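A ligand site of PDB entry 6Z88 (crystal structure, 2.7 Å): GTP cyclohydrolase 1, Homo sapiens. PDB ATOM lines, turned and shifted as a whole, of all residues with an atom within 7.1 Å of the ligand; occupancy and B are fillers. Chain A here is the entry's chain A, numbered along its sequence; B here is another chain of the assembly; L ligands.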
ATOM      1  N   VAL A 178     -29.881   4.941 -15.494  1.00  0.00           N
ATOM      2  CA  VAL A 178     -29.562   5.663 -16.724  1.00  0.00           C
ATOM      3  C   VAL A 178     -28.890   4.710 -17.729  1.00  0.00           C
ATOM      4  O   VAL A 178     -27.843   4.141 -17.448  1.00  0.00           O
ATOM      5  CB  VAL A 178     -28.671   6.896 -16.469  1.00  0.00           C
ATOM      6  CG1 VAL A 178     -28.361   7.624 -17.779  1.00  0.00           C
ATOM      7  CG2 VAL A 178     -29.314   7.841 -15.458  1.00  0.00           C
ATOM      8  N   THR A 201     -23.983   1.786 -22.071  1.00  0.00           N
ATOM      9  CA  THR A 201     -23.429   2.079 -20.758  1.00  0.00           C
ATOM     10  C   THR A 201     -24.608   2.269 -19.822  1.00  0.00           C
ATOM     11  O   THR A 201     -25.593   2.931 -20.182  1.00  0.00           O
ATOM     12  CB  THR A 201     -22.446   3.246 -20.798  1.00  0.00           C
ATOM     13  OG1 THR A 201     -23.089   4.431 -21.234  1.00  0.00           O
ATOM     14  CG2 THR A 201     -21.232   2.942 -21.667  1.00  0.00           C
ATOM     15  N   SER A 202     -24.557   1.623 -18.650  1.00  0.00           N
ATOM     16  CA  SER A 202     -25.689   1.619 -17.745  1.00  0.00           C
ATOM     17  C   SER A 202     -25.298   1.942 -16.309  1.00  0.00           C
ATOM     18  O   SER A 202     -24.442   1.277 -15.743  1.00  0.00           O
ATOM     19  CB  SER A 202     -26.359   0.249 -17.811  1.00  0.00           C
ATOM     20  OG  SER A 202     -27.408   0.084 -16.871  1.00  0.00           O
ATOM     21  N   THR A 203     -25.961   2.937 -15.696  1.00  0.00           N
ATOM     22  CA  THR A 203     -25.741   3.307 -14.297  1.00  0.00           C
ATOM     23  C   THR A 203     -26.979   2.969 -13.486  1.00  0.00           C
ATOM     24  O   THR A 203     -28.059   3.357 -13.879  1.00  0.00           O
ATOM     25  CB  THR A 203     -25.344   4.791 -14.145  1.00  0.00           C
ATOM     26  OG1 THR A 203     -24.032   4.945 -14.711  1.00  0.00           O
ATOM     27  CG2 THR A 203     -25.287   5.234 -12.698  1.00  0.00           C
ATOM     28  N   MET A 204     -26.847   2.186 -12.419  1.00  0.00           N
ATOM     29  CA  MET A 204     -27.978   1.849 -11.576  1.00  0.00           C
ATOM     30  C   MET A 204     -27.605   2.293 -10.157  1.00  0.00           C
ATOM     31  O   MET A 204     -26.628   1.795  -9.581  1.00  0.00           O
ATOM     32  CB  MET A 204     -28.222   0.329 -11.606  1.00  0.00           C
ATOM     33  CG  MET A 204     -28.543  -0.189 -12.972  1.00  0.00           C
ATOM     34  SD  MET A 204     -30.131   0.408 -13.578  1.00  0.00           S
ATOM     35  CE  MET A 204     -30.262  -0.490 -15.063  1.00  0.00           C
ATOM     36  N   LEU A 205     -28.320   3.282  -9.622  1.00  0.00           N
ATOM     37  CA  LEU A 205     -28.065   3.801  -8.290  1.00  0.00           C
ATOM     38  C   LEU A 205     -29.238   3.554  -7.365  1.00  0.00           C
ATOM     39  O   LEU A 205     -30.391   3.446  -7.805  1.00  0.00           O
ATOM     40  CB  LEU A 205     -27.763   5.298  -8.331  1.00  0.00           C
ATOM     41  CG  LEU A 205     -26.616   5.693  -9.226  1.00  0.00           C
ATOM     42  CD1 LEU A 205     -26.569   7.191  -9.408  1.00  0.00           C
ATOM     43  CD2 LEU A 205     -25.312   5.126  -8.712  1.00  0.00           C
ATOM     44  N   PHE A 208     -32.428   1.112  -7.554  1.00  0.00           N
ATOM     45  CA  PHE A 208     -32.239   0.604  -8.902  1.00  0.00           C
ATOM     46  C   PHE A 208     -31.067  -0.433  -8.935  1.00  0.00           C
ATOM     47  O   PHE A 208     -31.088  -1.378  -9.734  1.00  0.00           O
ATOM     48  CB  PHE A 208     -31.998   1.762  -9.880  1.00  0.00           C
ATOM     49  CG  PHE A 208     -33.238   2.389 -10.480  1.00  0.00           C
ATOM     50  CD1 PHE A 208     -34.112   3.126  -9.703  1.00  0.00           C
ATOM     51  CD2 PHE A 208     -33.552   2.220 -11.822  1.00  0.00           C
ATOM     52  CE1 PHE A 208     -35.229   3.729 -10.267  1.00  0.00           C
ATOM     53  CE2 PHE A 208     -34.664   2.840 -12.374  1.00  0.00           C
ATOM     54  CZ  PHE A 208     -35.523   3.540 -11.584  1.00  0.00           C
ATOM     55  N   ARG A 209     -30.062  -0.268  -8.063  1.00  0.00           N
ATOM     56  CA  ARG A 209     -28.943  -1.199  -7.969  1.00  0.00           C
ATOM     57  C   ARG A 209     -29.267  -2.304  -7.004  1.00  0.00           C
ATOM     58  O   ARG A 209     -28.980  -3.475  -7.270  1.00  0.00           O
ATOM     59  CB  ARG A 209     -27.673  -0.478  -7.506  1.00  0.00           C
ATOM     60  CG  ARG A 209     -26.484  -1.429  -7.391  1.00  0.00           C
ATOM     61  CD  ARG A 209     -25.195  -0.759  -7.021  1.00  0.00           C
ATOM     62  NE  ARG A 209     -24.905   0.318  -7.957  1.00  0.00           N
ATOM     63  CZ  ARG A 209     -23.751   0.971  -8.038  1.00  0.00           C
ATOM     64  NH1 ARG A 209     -23.607   1.958  -8.917  1.00  0.00           N
ATOM     65  NH2 ARG A 209     -22.736   0.630  -7.273  1.00  0.00           N
ATOM     66  N   ARG A 215     -34.820  -3.102 -10.700  1.00  0.00           N
ATOM     67  CA  ARG A 215     -33.982  -3.134 -11.903  1.00  0.00           C
ATOM     68  C   ARG A 215     -34.643  -3.903 -13.083  1.00  0.00           C
ATOM     69  O   ARG A 215     -34.561  -3.458 -14.242  1.00  0.00           O
ATOM     70  CB  ARG A 215     -32.564  -3.633 -11.581  1.00  0.00           C
ATOM     71  CG  ARG A 215     -31.520  -2.990 -12.501  1.00  0.00           C
ATOM     72  CD  ARG A 215     -30.180  -3.726 -12.462  1.00  0.00           C
ATOM     73  NE  ARG A 215     -29.544  -3.724 -11.139  1.00  0.00           N
ATOM     74  CZ  ARG A 215     -28.386  -4.300 -10.859  1.00  0.00           C
ATOM     75  NH1 ARG A 215     -27.666  -4.876 -11.817  1.00  0.00           N
ATOM     76  NH2 ARG A 215     -27.909  -4.268  -9.618  1.00  0.00           N
ATOM     77  N   ASP B 101     -18.097   3.251 -12.305  1.00  0.00           N
ATOM     78  CA  ASP B 101     -19.083   2.521 -11.508  1.00  0.00           C
ATOM     79  C   ASP B 101     -20.379   2.259 -12.311  1.00  0.00           C
ATOM     80  O   ASP B 101     -21.472   2.697 -11.928  1.00  0.00           O
ATOM     81  CB  ASP B 101     -19.407   3.303 -10.229  1.00  0.00           C
ATOM     82  CG  ASP B 101     -20.021   2.446  -9.141  1.00  0.00           C
ATOM     83  OD1 ASP B 101     -19.711   1.210  -9.115  1.00  0.00           O
ATOM     84  OD2 ASP B 101     -20.792   3.002  -8.305  1.00  0.00           O
ATOM     85  N   GLU B 102     -20.246   1.550 -13.437  1.00  0.00           N
ATOM     86  CA  GLU B 102     -21.361   1.281 -14.339  1.00  0.00           C
ATOM     87  C   GLU B 102     -21.048   0.139 -15.255  1.00  0.00           C
ATOM     88  O   GLU B 102     -19.886  -0.121 -15.560  1.00  0.00           O
ATOM     89  CB  GLU B 102     -21.660   2.523 -15.172  1.00  0.00           C
ATOM     90  CG  GLU B 102     -20.475   3.090 -15.905  1.00  0.00           C
ATOM     91  CD  GLU B 102     -20.773   4.465 -16.467  1.00  0.00           C
ATOM     92  OE1 GLU B 102     -21.461   4.533 -17.507  1.00  0.00           O
ATOM     93  OE2 GLU B 102     -20.349   5.466 -15.836  1.00  0.00           O
ATOM     94  N   MET B 103     -22.085  -0.541 -15.741  1.00  0.00           N
ATOM     95  CA  MET B 103     -21.888  -1.643 -16.661  1.00  0.00           C
ATOM     96  C   MET B 103     -21.517  -1.104 -18.052  1.00  0.00           C
ATOM     97  O   MET B 103     -22.165  -0.188 -18.548  1.00  0.00           O
ATOM     98  CB  MET B 103     -23.105  -2.550 -16.714  1.00  0.00           C
ATOM     99  CG  MET B 103     -22.835  -3.763 -17.517  1.00  0.00           C
ATOM    100  SD  MET B 103     -24.186  -4.913 -17.482  1.00  0.00           S
ATOM    101  CE  MET B 103     -24.078  -5.445 -15.825  1.00  0.00           C
ATOM    102  N   VAL B 104     -20.450  -1.639 -18.635  1.00  0.00           N
ATOM    103  CA  VAL B 104     -20.024  -1.218 -19.962  1.00  0.00           C
ATOM    104  C   VAL B 104     -20.189  -2.377 -20.952  1.00  0.00           C
ATOM    105  O   VAL B 104     -19.581  -3.431 -20.764  1.00  0.00           O
ATOM    106  CB  VAL B 104     -18.595  -0.636 -19.948  1.00  0.00           C
ATOM    107  CG1 VAL B 104     -18.118  -0.319 -21.350  1.00  0.00           C
ATOM    108  CG2 VAL B 104     -18.528   0.605 -19.056  1.00  0.00           C
ATOM    109  N   LEU B 131     -17.940  -4.834 -15.596  1.00  0.00           N
ATOM    110  CA  LEU B 131     -18.127  -3.861 -14.539  1.00  0.00           C
ATOM    111  C   LEU B 131     -16.736  -3.534 -14.069  1.00  0.00           C
ATOM    112  O   LEU B 131     -16.057  -4.408 -13.558  1.00  0.00           O
ATOM    113  CB  LEU B 131     -18.920  -4.473 -13.410  1.00  0.00           C
ATOM    114  CG  LEU B 131     -20.383  -4.221 -13.499  1.00  0.00           C
ATOM    115  CD1 LEU B 131     -21.143  -5.156 -12.607  1.00  0.00           C
ATOM    116  CD2 LEU B 131     -20.676  -2.776 -13.181  1.00  0.00           C
ATOM    117  N   PRO B 132     -16.233  -2.309 -14.332  1.00  0.00           N
ATOM    118  CA  PRO B 132     -14.841  -2.006 -13.969  1.00  0.00           C
ATOM    119  C   PRO B 132     -14.606  -1.905 -12.479  1.00  0.00           C
ATOM    120  O   PRO B 132     -15.516  -1.603 -11.729  1.00  0.00           O
ATOM    121  CB  PRO B 132     -14.564  -0.665 -14.660  1.00  0.00           C
ATOM    122  CG  PRO B 132     -15.734  -0.392 -15.547  1.00  0.00           C
ATOM    123  CD  PRO B 132     -16.884  -1.167 -14.989  1.00  0.00           C
ATOM    124  N   ALA B 174     -14.669  -6.145 -11.770  1.00  0.00           N
ATOM    125  CA  ALA B 174     -15.549  -6.823 -10.809  1.00  0.00           C
ATOM    126  C   ALA B 174     -16.206  -8.067 -11.465  1.00  0.00           C
ATOM    127  O   ALA B 174     -16.406  -9.086 -10.812  1.00  0.00           O
ATOM    128  CB  ALA B 174     -16.606  -5.859 -10.320  1.00  0.00           C
ATOM    129  N   VAL B 207     -18.751 -10.890 -10.730  1.00  0.00           N
ATOM    130  CA  VAL B 207     -20.075 -10.386 -10.407  1.00  0.00           C
ATOM    131  C   VAL B 207     -21.114 -10.767 -11.500  1.00  0.00           C
ATOM    132  O   VAL B 207     -22.290 -10.954 -11.177  1.00  0.00           O
ATOM    133  CB  VAL B 207     -19.967  -8.886 -10.124  1.00  0.00           C
ATOM    134  CG1 VAL B 207     -21.300  -8.159 -10.248  1.00  0.00           C
ATOM    135  CG2 VAL B 207     -19.368  -8.654  -8.754  1.00  0.00           C
ATOM    136  N   PHE B 208     -20.664 -10.975 -12.774  1.00  0.00           N
ATOM    137  CA  PHE B 208     -21.573 -11.432 -13.842  1.00  0.00           C
ATOM    138  C   PHE B 208     -22.045 -12.854 -13.568  1.00  0.00           C
ATOM    139  O   PHE B 208     -23.189 -13.184 -13.876  1.00  0.00           O
ATOM    140  CB  PHE B 208     -20.918 -11.349 -15.222  1.00  0.00           C
ATOM    141  CG  PHE B 208     -20.939  -9.973 -15.880  1.00  0.00           C
ATOM    142  CD1 PHE B 208     -20.324  -8.889 -15.271  1.00  0.00           C
ATOM    143  CD2 PHE B 208     -21.550  -9.778 -17.107  1.00  0.00           C
ATOM    144  CE1 PHE B 208     -20.325  -7.642 -15.874  1.00  0.00           C
ATOM    145  CE2 PHE B 208     -21.549  -8.521 -17.709  1.00  0.00           C
ATOM    146  CZ  PHE B 208     -20.948  -7.467 -17.083  1.00  0.00           C
ATOM    147  N   ASP B 211     -23.811 -12.383  -9.350  1.00  0.00           N
ATOM    148  CA  ASP B 211     -24.958 -11.491  -9.112  1.00  0.00           C
ATOM    149  C   ASP B 211     -26.041 -11.737 -10.135  1.00  0.00           C
ATOM    150  O   ASP B 211     -25.842 -11.493 -11.323  1.00  0.00           O
ATOM    151  CB  ASP B 211     -24.516 -10.031  -9.132  1.00  0.00           C
ATOM    152  CG  ASP B 211     -25.504  -9.034  -8.561  1.00  0.00           C
ATOM    153  OD1 ASP B 211     -26.667  -9.395  -8.404  1.00  0.00           O
ATOM    154  OD2 ASP B 211     -25.104  -7.882  -8.298  1.00  0.00           O
ATOM    155  N   LYS B 213     -28.771  -9.995 -10.579  1.00  0.00           N
ATOM    156  CA  LYS B 213     -29.143  -8.690 -11.117  1.00  0.00           C
ATOM    157  C   LYS B 213     -28.186  -8.314 -12.254  1.00  0.00           C
ATOM    158  O   LYS B 213     -28.638  -7.914 -13.314  1.00  0.00           O
ATOM    159  CB  LYS B 213     -29.077  -7.618 -10.023  1.00  0.00           C
ATOM    160  CG  LYS B 213     -29.978  -7.858  -8.845  1.00  0.00           C
ATOM    161  CD  LYS B 213     -29.910  -6.716  -7.860  1.00  0.00           C
ATOM    162  CE  LYS B 213     -29.275  -7.152  -6.598  1.00  0.00           C
ATOM    163  NZ  LYS B 213     -27.886  -7.553  -6.827  1.00  0.00           N
ATOM    164  N   THR B 214     -26.873  -8.479 -12.033  1.00  0.00           N
ATOM    165  CA  THR B 214     -25.851  -8.174 -13.026  1.00  0.00           C
ATOM    166  C   THR B 214     -25.994  -9.023 -14.286  1.00  0.00           C
ATOM    167  O   THR B 214     -25.954  -8.473 -15.392  1.00  0.00           O
ATOM    168  CB  THR B 214     -24.450  -8.352 -12.417  1.00  0.00           C
ATOM    169  OG1 THR B 214     -24.306  -7.428 -11.357  1.00  0.00           O
ATOM    170  CG2 THR B 214     -23.360  -8.077 -13.391  1.00  0.00           C
ATOM    171  N   ARG B 215     -26.172 -10.350 -14.132  1.00  0.00           N
ATOM    172  CA  ARG B 215     -26.297 -11.218 -15.306  1.00  0.00           C
ATOM    173  C   ARG B 215     -27.579 -10.940 -16.121  1.00  0.00           C
ATOM    174  O   ARG B 215     -27.525 -10.902 -17.365  1.00  0.00           O
ATOM    175  CB  ARG B 215     -26.162 -12.709 -14.934  1.00  0.00           C
ATOM    176  CG  ARG B 215     -25.575 -13.544 -16.083  1.00  0.00           C
ATOM    177  CD  ARG B 215     -25.757 -15.040 -15.909  1.00  0.00           C
ATOM    178  NE  ARG B 215     -25.038 -15.593 -14.759  1.00  0.00           N
ATOM    179  CZ  ARG B 215     -25.038 -16.879 -14.419  1.00  0.00           C
ATOM    180  NH1 ARG B 215     -25.742 -17.751 -15.113  1.00  0.00           N
ATOM    181  NH2 ARG B 215     -24.344 -17.294 -13.373  1.00  0.00           N
ATOM    182  N   GLU B 217     -29.234  -8.116 -16.302  1.00  0.00           N
ATOM    183  CA  GLU B 217     -28.982  -6.831 -16.930  1.00  0.00           C
ATOM    184  C   GLU B 217     -28.123  -6.935 -18.170  1.00  0.00           C
ATOM    185  O   GLU B 217     -28.491  -6.363 -19.194  1.00  0.00           O
ATOM    186  CB  GLU B 217     -28.317  -5.900 -15.915  1.00  0.00           C
ATOM    187  CG  GLU B 217     -27.952  -4.534 -16.446  1.00  0.00           C
ATOM    188  CD  GLU B 217     -27.387  -3.603 -15.411  1.00  0.00           C
ATOM    189  OE1 GLU B 217     -27.150  -2.417 -15.740  1.00  0.00           O
ATOM    190  OE2 GLU B 217     -27.151  -4.050 -14.260  1.00  0.00           O
ATOM    191  N   LEU B 221     -29.621  -6.163 -21.886  1.00  0.00           N
ATOM    192  CA  LEU B 221     -29.076  -5.035 -22.620  1.00  0.00           C
ATOM    193  C   LEU B 221     -28.434  -5.431 -23.926  1.00  0.00           C
ATOM    194  O   LEU B 221     -28.412  -4.607 -24.835  1.00  0.00           O
ATOM    195  CB  LEU B 221     -28.132  -4.198 -21.759  1.00  0.00           C
ATOM    196  CG  LEU B 221     -28.809  -3.459 -20.591  1.00  0.00           C
ATOM    197  CD1 LEU B 221     -27.794  -2.790 -19.696  1.00  0.00           C
ATOM    198  CD2 LEU B 221     -29.814  -2.440 -21.066  1.00  0.00           C
HETATM  199  C1  LIG L   1     -24.523  -3.680 -11.960  1.00  0.00           C
HETATM  200  C2  LIG L   1     -22.262  -2.546  -9.403  1.00  0.00           C
HETATM  201  C3  LIG L   1     -24.753  -1.594 -13.202  1.00  0.00           C
HETATM  202  N1  LIG L   1     -25.293  -0.999 -14.238  1.00  0.00           N
HETATM  203  C4  LIG L   1     -23.421  -1.568 -11.405  1.00  0.00           C
HETATM  204  C5  LIG L   1     -23.651  -2.939 -11.101  1.00  0.00           C
HETATM  205  S1  LIG L   1     -22.307  -0.937 -10.240  1.00  0.00           S
HETATM  206  N2  LIG L   1     -23.938  -0.893 -12.397  1.00  0.00           N
HETATM  207  N3  LIG L   1     -23.036  -3.496 -10.024  1.00  0.00           N
HETATM  208  N4  LIG L   1     -25.042  -2.907 -12.974  1.00  0.00           N
HETATM  209  O1  LIG L   1     -24.883  -4.848 -11.811  1.00  0.00           O
HETATM  210  O2  LIG L   1     -21.593  -2.718  -8.401  1.00  0.00           O
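OG1 of Thr 214 of chain B lies within hydrogen-bond range of O1 of the ligand, 2.7 Å away.
N4 of the ligand lies within hydrogen-bond range of OE2 of Glu 217 of chain B, at 2.7 Å.
N1 of the ligand sits at hydrogen-bond distance from O of Ser 202 (2.9 Å).
The guanidinium group (NH2) of Arg 209 sits close to a sulfur (S1) of the ligand.
An oxygen (O1) of the ligand sits at hydrogen-bond distance from the guanidinium group of Arg 215 of chain A.
NE of Arg 209 lies within hydrogen-bond range of O of Met 204 (2.8 Å).
The guanidinium group of Arg 209 lies within salt-bridge range of the side-chain carboxylate of Asp 101 of chain B (3.1 Å).
The backbone carbonyl oxygen of Phe 208 of chain A sits at hydrogen-bond distance from the guanidinium group of Arg 215 of chain A (3.1 Å).
N of Met 103 of chain B is in hydrogen-bond range of O of Ser 202 (3.0 Å).
OG of Ser 202 is in hydrogen-bond range of OE1 of Glu 217 of chain B, at 2.8 Å.
The side-chain hydroxyl of Thr 214 of chain B sits at hydrogen-bond distance from the side-chain carboxylate of Asp 211 of chain B, 3.2 Å away.
OE2 of Glu 217 of chain B lies within salt-bridge range of NH1 of Arg 215 of chain A.
NH2 of Arg 215 of chain A sits at hydrogen-bond distance from O of Arg 209 (2.7 Å).
OD1 of Asp 101 of chain B lies close to S1 of the ligand.
Residues that only touch the ligand: Met 204 (3.6 Å), Glu 102 of chain B (3.9 Å), Met 103 of chain B (3.6 Å) and Leu 131 of chain B (3.5 Å).
Hydrophobic or aromatic side chains that line the ligand: Met 204, Met 103 of chain B and Leu 131 of chain B.
Ten residues have an atom within 4 Å of the ligand: Ser 202, Met 204, Arg 209, Arg 215 of chain A, Asp 101 of chain B, Glu 102 of chain B, Met 103 of chain B, Leu 131 of chain B, Thr 214 of chain B and Glu 217 of chain B.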
